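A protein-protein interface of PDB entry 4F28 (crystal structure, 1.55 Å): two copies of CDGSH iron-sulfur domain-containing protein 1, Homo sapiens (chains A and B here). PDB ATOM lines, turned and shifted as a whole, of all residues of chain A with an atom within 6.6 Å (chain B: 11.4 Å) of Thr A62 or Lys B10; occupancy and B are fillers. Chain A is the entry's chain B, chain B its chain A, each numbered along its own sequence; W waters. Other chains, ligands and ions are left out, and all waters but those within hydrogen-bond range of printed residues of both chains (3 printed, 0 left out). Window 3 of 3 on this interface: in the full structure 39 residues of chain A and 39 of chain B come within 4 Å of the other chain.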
ATOM      1  N   ARG A  44      -5.952  17.644  10.848  1.00  0.00           N
ATOM      2  CA  ARG A  44      -5.462  19.015  11.002  1.00  0.00           C
ATOM      3  C   ARG A  44      -5.125  19.639   9.653  1.00  0.00           C
ATOM      4  O   ARG A  44      -4.944  20.865   9.563  1.00  0.00           O
ATOM      5  CB  ARG A  44      -4.230  19.085  11.933  1.00  0.00           C
ATOM      6  CG  ARG A  44      -4.456  18.606  13.367  1.00  0.00           C
ATOM      7  CD  ARG A  44      -5.422  19.482  14.161  1.00  0.00           C
ATOM      8  NE  ARG A  44      -5.586  18.940  15.505  1.00  0.00           N
ATOM      9  CZ  ARG A  44      -6.507  18.042  15.828  1.00  0.00           C
ATOM     10  NH1 ARG A  44      -7.370  17.607  14.916  1.00  0.00           N
ATOM     11  NH2 ARG A  44      -6.561  17.557  17.059  1.00  0.00           N
ATOM     12  N   LYS A  57       3.324  20.079  12.779  1.00  0.00           N
ATOM     13  CA  LYS A  57       2.954  21.077  13.770  1.00  0.00           C
ATOM     14  C   LYS A  57       2.208  20.415  14.933  1.00  0.00           C
ATOM     15  O   LYS A  57       2.534  20.711  16.083  1.00  0.00           O
ATOM     16  CB  LYS A  57       2.120  22.195  13.121  1.00  0.00           C
ATOM     17  CG  LYS A  57       1.760  23.361  14.038  1.00  0.00           C
ATOM     18  CD  LYS A  57       0.940  24.403  13.288  1.00  0.00           C
ATOM     19  CE  LYS A  57       0.325  25.461  14.178  1.00  0.00           C
ATOM     20  NZ  LYS A  57      -1.042  25.084  14.637  1.00  0.00           N
ATOM     21  N   HIS A  58       1.239  19.502  14.640  1.00  0.00           N
ATOM     22  CA  HIS A  58       0.474  18.801  15.679  1.00  0.00           C
ATOM     23  C   HIS A  58       1.417  18.008  16.615  1.00  0.00           C
ATOM     24  O   HIS A  58       1.317  18.130  17.836  1.00  0.00           O
ATOM     25  CB  HIS A  58      -0.582  17.848  15.060  1.00  0.00           C
ATOM     26  CG  HIS A  58      -1.124  16.876  16.059  1.00  0.00           C
ATOM     27  ND1 HIS A  58      -2.088  17.255  16.978  1.00  0.00           N
ATOM     28  CD2 HIS A  58      -0.755  15.597  16.306  1.00  0.00           C
ATOM     29  CE1 HIS A  58      -2.291  16.192  17.739  1.00  0.00           C
ATOM     30  NE2 HIS A  58      -1.517  15.163  17.364  1.00  0.00           N
ATOM     31  N   ASN A  59       2.305  17.181  16.030  1.00  0.00           N
ATOM     32  CA  ASN A  59       3.249  16.365  16.789  1.00  0.00           C
ATOM     33  C   ASN A  59       4.146  17.217  17.694  1.00  0.00           C
ATOM     34  O   ASN A  59       4.306  16.875  18.858  1.00  0.00           O
ATOM     35  CB  ASN A  59       4.094  15.522  15.856  1.00  0.00           C
ATOM     36  CG  ASN A  59       3.297  14.405  15.226  1.00  0.00           C
ATOM     37  OD1 ASN A  59       2.202  14.030  15.694  1.00  0.00           O
ATOM     38  ND2 ASN A  59       3.842  13.849  14.149  1.00  0.00           N
ATOM     39  N   GLU A  60       4.677  18.331  17.178  1.00  0.00           N
ATOM     40  CA  GLU A  60       5.552  19.244  17.935  1.00  0.00           C
ATOM     41  C   GLU A  60       4.802  19.891  19.111  1.00  0.00           C
ATOM     42  O   GLU A  60       5.317  19.875  20.221  1.00  0.00           O
ATOM     43  CB  GLU A  60       6.133  20.321  17.003  1.00  0.00           C
ATOM     44  CG  GLU A  60       7.397  20.999  17.511  1.00  0.00           C
ATOM     45  CD  GLU A  60       7.772  22.269  16.771  1.00  0.00           C
ATOM     46  OE1 GLU A  60       6.888  22.858  16.105  1.00  0.00           O
ATOM     47  OE2 GLU A  60       8.938  22.710  16.904  1.00  0.00           O
ATOM     48  N   GLU A  61       3.572  20.393  18.886  1.00  0.00           N
ATOM     49  CA  GLU A  61       2.777  21.060  19.921  1.00  0.00           C
ATOM     50  C   GLU A  61       2.220  20.112  21.000  1.00  0.00           C
ATOM     51  O   GLU A  61       1.958  20.567  22.111  1.00  0.00           O
ATOM     52  CB  GLU A  61       1.593  21.820  19.282  1.00  0.00           C
ATOM     53  CG  GLU A  61       2.007  23.035  18.463  1.00  0.00           C
ATOM     54  CD  GLU A  61       0.888  23.771  17.748  1.00  0.00           C
ATOM     55  OE1 GLU A  61      -0.032  23.108  17.213  1.00  0.00           O
ATOM     56  OE2 GLU A  61       0.958  25.020  17.686  1.00  0.00           O
ATOM     57  N   THR A  62       1.994  18.825  20.674  1.00  0.00           N
ATOM     58  CA  THR A  62       1.340  17.883  21.594  1.00  0.00           C
ATOM     59  C   THR A  62       2.243  16.758  22.118  1.00  0.00           C
ATOM     60  O   THR A  62       1.871  16.096  23.088  1.00  0.00           O
ATOM     61  CB  THR A  62       0.111  17.243  20.910  1.00  0.00           C
ATOM     62  OG1 THR A  62       0.538  16.487  19.777  1.00  0.00           O
ATOM     63  CG2 THR A  62      -0.928  18.265  20.463  1.00  0.00           C
ATOM     64  N   GLY A  63       3.362  16.502  21.440  1.00  0.00           N
ATOM     65  CA  GLY A  63       4.260  15.400  21.770  1.00  0.00           C
ATOM     66  C   GLY A  63       3.825  14.100  21.109  1.00  0.00           C
ATOM     67  O   GLY A  63       4.374  13.037  21.419  1.00  0.00           O
ATOM     68  N   ASP A  64       2.851  14.180  20.165  1.00  0.00           N
ATOM     69  CA  ASP A  64       2.315  13.042  19.438  1.00  0.00           C
ATOM     70  C   ASP A  64       3.293  12.533  18.351  1.00  0.00           C
ATOM     71  O   ASP A  64       4.346  13.141  18.099  1.00  0.00           O
ATOM     72  CB  ASP A  64       0.948  13.407  18.799  1.00  0.00           C
ATOM     73  CG  ASP A  64      -0.035  12.265  18.681  1.00  0.00           C
ATOM     74  OD1 ASP A  64       0.366  11.104  18.934  1.00  0.00           O
ATOM     75  OD2 ASP A  64      -1.227  12.536  18.362  1.00  0.00           O
ATOM     76  N   ASN A  65       2.924  11.419  17.700  1.00  0.00           N
ATOM     77  CA  ASN A  65       3.744  10.747  16.691  1.00  0.00           C
ATOM     78  C   ASN A  65       2.872  10.249  15.507  1.00  0.00           C
ATOM     79  O   ASN A  65       3.121   9.163  14.946  1.00  0.00           O
ATOM     80  CB  ASN A  65       4.480   9.571  17.364  1.00  0.00           C
ATOM     81  CG  ASN A  65       3.552   8.456  17.820  1.00  0.00           C
ATOM     82  OD1 ASN A  65       2.380   8.672  18.125  1.00  0.00           O
ATOM     83  ND2 ASN A  65       4.032   7.226  17.777  1.00  0.00           N
ATOM     84  N   LYS B  10      -3.240  20.756  21.712  1.00  0.00           N
ATOM     85  CA  LYS B  10      -2.795  20.376  23.052  1.00  0.00           C
ATOM     86  C   LYS B  10      -2.931  18.866  23.282  1.00  0.00           C
ATOM     87  O   LYS B  10      -1.956  18.216  23.675  1.00  0.00           O
ATOM     88  N   ALA B  11      -4.129  18.315  23.026  1.00  0.00           N
ATOM     89  CA  ALA B  11      -4.422  16.898  23.216  1.00  0.00           C
ATOM     90  C   ALA B  11      -3.816  16.027  22.111  1.00  0.00           C
ATOM     91  O   ALA B  11      -3.900  16.364  20.925  1.00  0.00           O
ATOM     92  CB  ALA B  11      -5.930  16.679  23.268  1.00  0.00           C
ATOM     93  N   MET B  12      -3.213  14.896  22.507  1.00  0.00           N
ATOM     94  CA  MET B  12      -2.668  13.926  21.558  1.00  0.00           C
ATOM     95  C   MET B  12      -3.822  13.215  20.856  1.00  0.00           C
ATOM     96  O   MET B  12      -4.907  13.073  21.433  1.00  0.00           O
ATOM     97  CB  MET B  12      -1.772  12.897  22.253  1.00  0.00           C
ATOM     98  CG  MET B  12      -0.421  13.425  22.680  1.00  0.00           C
ATOM     99  SD  MET B  12       0.829  12.109  22.819  1.00  0.00           S
ATOM    100  CE  MET B  12       0.128  11.071  24.074  1.00  0.00           C
ATOM    101  N   ILE B  13      -3.604  12.797  19.609  1.00  0.00           N
ATOM    102  CA  ILE B  13      -4.589  12.060  18.821  1.00  0.00           C
ATOM    103  C   ILE B  13      -4.323  10.575  19.038  1.00  0.00           C
ATOM    104  O   ILE B  13      -5.240   9.815  19.364  1.00  0.00           O
ATOM    105  CB  ILE B  13      -4.489  12.495  17.339  1.00  0.00           C
ATOM    106  CG1 ILE B  13      -5.049  13.922  17.175  1.00  0.00           C
ATOM    107  CG2 ILE B  13      -5.128  11.458  16.390  1.00  0.00           C
ATOM    108  CD1 ILE B  13      -4.623  14.660  15.950  1.00  0.00           C
ATOM    109  N   ASN B  14      -3.042  10.172  18.880  1.00  0.00           N
ATOM    110  CA  ASN B  14      -2.657   8.791  19.111  1.00  0.00           C
ATOM    111  C   ASN B  14      -2.240   8.659  20.566  1.00  0.00           C
ATOM    112  O   ASN B  14      -1.349   9.391  21.023  1.00  0.00           O
ATOM    113  CB  ASN B  14      -1.524   8.348  18.164  1.00  0.00           C
ATOM    114  CG  ASN B  14      -1.017   6.949  18.430  1.00  0.00           C
ATOM    115  OD1 ASN B  14      -1.772   6.074  18.856  1.00  0.00           O
ATOM    116  ND2 ASN B  14       0.272   6.687  18.162  1.00  0.00           N
ATOM    117  N   LEU B  15      -2.862   7.714  21.292  1.00  0.00           N
ATOM    118  CA  LEU B  15      -2.511   7.555  22.704  1.00  0.00           C
ATOM    119  C   LEU B  15      -1.659   6.323  23.014  1.00  0.00           C
ATOM    120  O   LEU B  15      -0.857   6.409  23.947  1.00  0.00           O
ATOM    121  CB  LEU B  15      -3.776   7.498  23.600  1.00  0.00           C
ATOM    122  CG  LEU B  15      -4.843   8.610  23.456  1.00  0.00           C
ATOM    123  CD1 LEU B  15      -6.139   8.228  24.173  1.00  0.00           C
ATOM    124  CD2 LEU B  15      -4.343   9.932  23.993  1.00  0.00           C
ATOM    125  N   LYS B  19       4.438   3.804  20.219  1.00  0.00           N
ATOM    126  CA  LYS B  19       4.962   5.053  20.783  1.00  0.00           C
ATOM    127  C   LYS B  19       6.509   5.164  20.671  1.00  0.00           C
ATOM    128  O   LYS B  19       7.044   6.277  20.850  1.00  0.00           O
ATOM    129  CB  LYS B  19       4.447   5.304  22.206  1.00  0.00           C
ATOM    130  CG  LYS B  19       2.995   5.858  22.226  1.00  0.00           C
ATOM    131  CD  LYS B  19       2.865   7.237  21.548  1.00  0.00           C
ATOM    132  CE  LYS B  19       1.427   7.705  21.373  1.00  0.00           C
ATOM    133  NZ  LYS B  19       1.401   9.109  20.875  1.00  0.00           N
ATOM    134  N   PRO B  22       8.789   7.704  16.311  1.00  0.00           N
ATOM    135  CA  PRO B  22       8.541   9.157  16.475  1.00  0.00           C
ATOM    136  C   PRO B  22       7.548   9.747  15.490  1.00  0.00           C
ATOM    137  O   PRO B  22       7.042  10.840  15.745  1.00  0.00           O
ATOM    138  CB  PRO B  22       9.913   9.783  16.260  1.00  0.00           C
ATOM    139  CG  PRO B  22      10.671   8.797  15.466  1.00  0.00           C
ATOM    140  CD  PRO B  22      10.173   7.440  15.870  1.00  0.00           C
ATOM    141  N   LYS B  23       7.244   9.044  14.368  1.00  0.00           N
ATOM    142  CA  LYS B  23       6.249   9.528  13.402  1.00  0.00           C
ATOM    143  C   LYS B  23       5.748   8.344  12.609  1.00  0.00           C
ATOM    144  O   LYS B  23       6.520   7.799  11.808  1.00  0.00           O
ATOM    145  CB  LYS B  23       6.831  10.619  12.483  1.00  0.00           C
ATOM    146  CG  LYS B  23       5.751  11.151  11.507  1.00  0.00           C
ATOM    147  CD  LYS B  23       6.284  12.255  10.604  1.00  0.00           C
ATOM    148  CE  LYS B  23       7.401  11.800   9.683  1.00  0.00           C
ATOM    149  NZ  LYS B  23       7.906  12.897   8.823  1.00  0.00           N
ATOM    150  N   TRP B  43      -6.829   6.100  15.094  1.00  0.00           N
ATOM    151  CA  TRP B  43      -5.726   5.664  15.974  1.00  0.00           C
ATOM    152  C   TRP B  43      -6.249   4.925  17.237  1.00  0.00           C
ATOM    153  O   TRP B  43      -5.612   4.969  18.298  1.00  0.00           O
ATOM    154  CB  TRP B  43      -4.843   6.883  16.351  1.00  0.00           C
ATOM    155  CG  TRP B  43      -4.282   7.595  15.159  1.00  0.00           C
ATOM    156  CD1 TRP B  43      -4.917   8.514  14.379  1.00  0.00           C
ATOM    157  CD2 TRP B  43      -3.024   7.334  14.530  1.00  0.00           C
ATOM    158  NE1 TRP B  43      -4.103   8.898  13.344  1.00  0.00           N
ATOM    159  CE2 TRP B  43      -2.939   8.183  13.403  1.00  0.00           C
ATOM    160  CE3 TRP B  43      -1.928   6.514  14.853  1.00  0.00           C
ATOM    161  CZ2 TRP B  43      -1.812   8.219  12.579  1.00  0.00           C
ATOM    162  CZ3 TRP B  43      -0.815   6.544  14.039  1.00  0.00           C
ATOM    163  CH2 TRP B  43      -0.744   7.405  12.934  1.00  0.00           C
ATOM    164  N   ARG B  44      -7.398   4.218  17.110  1.00  0.00           N
ATOM    165  CA  ARG B  44      -7.989   3.431  18.197  1.00  0.00           C
ATOM    166  C   ARG B  44      -8.120   1.968  17.777  1.00  0.00           C
ATOM    167  O   ARG B  44      -8.357   1.120  18.628  1.00  0.00           O
ATOM    168  CB  ARG B  44      -9.353   3.995  18.655  1.00  0.00           C
ATOM    169  CG  ARG B  44      -9.311   5.419  19.201  1.00  0.00           C
ATOM    170  CD  ARG B  44      -8.538   5.598  20.507  1.00  0.00           C
ATOM    171  NE  ARG B  44      -8.562   7.007  20.920  1.00  0.00           N
ATOM    172  CZ  ARG B  44      -7.678   7.924  20.533  1.00  0.00           C
ATOM    173  NH1 ARG B  44      -6.649   7.583  19.766  1.00  0.00           N
ATOM    174  NH2 ARG B  44      -7.810   9.189  20.925  1.00  0.00           N
HETATM  175  O   HOH W   1      -5.387  18.104  19.554  1.00  0.00           O
HETATM  176  O   HOH W   2      -7.033  15.996  19.474  1.00  0.00           O
HETATM  177  O   HOH W   3       3.832  10.521  21.272  1.00  0.00           O
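Among the printed residues, merely in contact across the chains: Arg A44 with Ile B13, His A58 with Ala B11, His A58 with Ile B13, Thr A62 with Lys B10, Thr A62 with Ala B11, Thr A62 with Met B12, Gly A63 with Met B12, Asp A64 with Met B12, Asn A65 with Pro B22 and Asn A65 with Lys B23.
Of the 10 printed residues of chain A, 6 touch a printed residue of chain B.
Printed residues of chain A that touch a printed residue of chain B: Arg A44, His A58, Thr A62, Gly A63, Asp A64 and Asn A65.
Hydrophobic or aromatic side chains of chain A within 4 Å of the printed part of chain B: His A58.
Hydrophobic or aromatic side chains of chain B that line the printed part of chain A: Met B12 and Ile B13.
Along chain B the printed residues that touch a printed residue of chain A span positions 10 to 23.
Among the printed residues, 15 pairs touch across the chains.
Among the printed residues, Asp or Glu carboxylates within 4 Å of a Lys or Arg side-chain nitrogen of the other chain: Asp A64 with Lys B19 (3.0 Å).
Water W3 lies within hydrogen-bond range of O of Gly A63, NZ of Lys B19 and SD of Met B12.
Water W1 bridges the backbone carbonyl oxygen of Ala B11 (2.7 Å) and the guanidinium group of Arg A44 (2.8 Å).
Water W2 bridges NH2 of Arg A44 and O of Ala B11.
Of the printed residues of chain B, Thr A62 touches Lys B10 (3.4 Å), Ala B11 (3.6 Å) and Met B12 (3.5 Å).
Lys B10 touches one residue of chain A.
No residue of chain B comes within 4 Å of Glu A61.
Of the printed residues of chain B, Gly A63 touches Met B12 (3.9 Å).
Of the printed residues of chain A, Lys B23 touches Asn A65 (3.5 Å).
Of the printed residues of chain B, Asn A65 touches Asn B14 (2.9 Å), Lys B19 (3.0 Å), Pro B22 (3.3 Å) and Lys B23 (3.5 Å).
Printed residues of chain A within 4 Å of Lys B19: Asp A64 (3.0 Å) and Asn A65 (3.0 Å).
Printed residues of chain A within 4 Å of Met B12: Thr A62, Gly A63 and Asp A64.
The nearest residue of chain B that does not touch Thr A62 is Ile B13 (5.5 Å).
OD2 of Asp A64 sits at hydrogen-bond distance from N of Ile B13, 2.7 Å away.
The side-chain carboxylate of Asp A64 is in hydrogen-bond range of the backbone NH of Asn B14 (3.0 Å).
ND2 of Asn B14 sits at hydrogen-bond distance from OD1 of Asn A65 (2.9 Å).
OD1 of Asp A64 is in salt-bridge range of NZ of Lys B19.
The side-chain amide oxygen (OD1) of Asn A65 sits at hydrogen-bond distance from the side-chain amino group (NZ) of Lys B19, at 3.0 Å.
Position printed for both chains: 44.
Of the 15 pairs that touch across the chains among the printed residues, none has its exchanged pair printed and touching as well.
SD of Met B12 is in hydrogen-bond range of NZ of Lys B19, at 3.6 Å.
O of Ile B13 sits at hydrogen-bond distance from NH1 of Arg B44 (2.7 Å).
O of His A58 lies within hydrogen-bond range of OG1 of Thr A62 (2.7 Å).
The side-chain amide oxygen (OD1) of Asn A59 sits at hydrogen-bond distance from the backbone NH (N) of Asn A65, 3.4 Å away.
OG1 of Thr A62 lies close to N of Asp A64 (3.3 Å).
The side-chain carboxylate (OD1) of Asp A64 lies close to the side-chain amide oxygen (OD1) of Asn A65 (3.3 Å).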
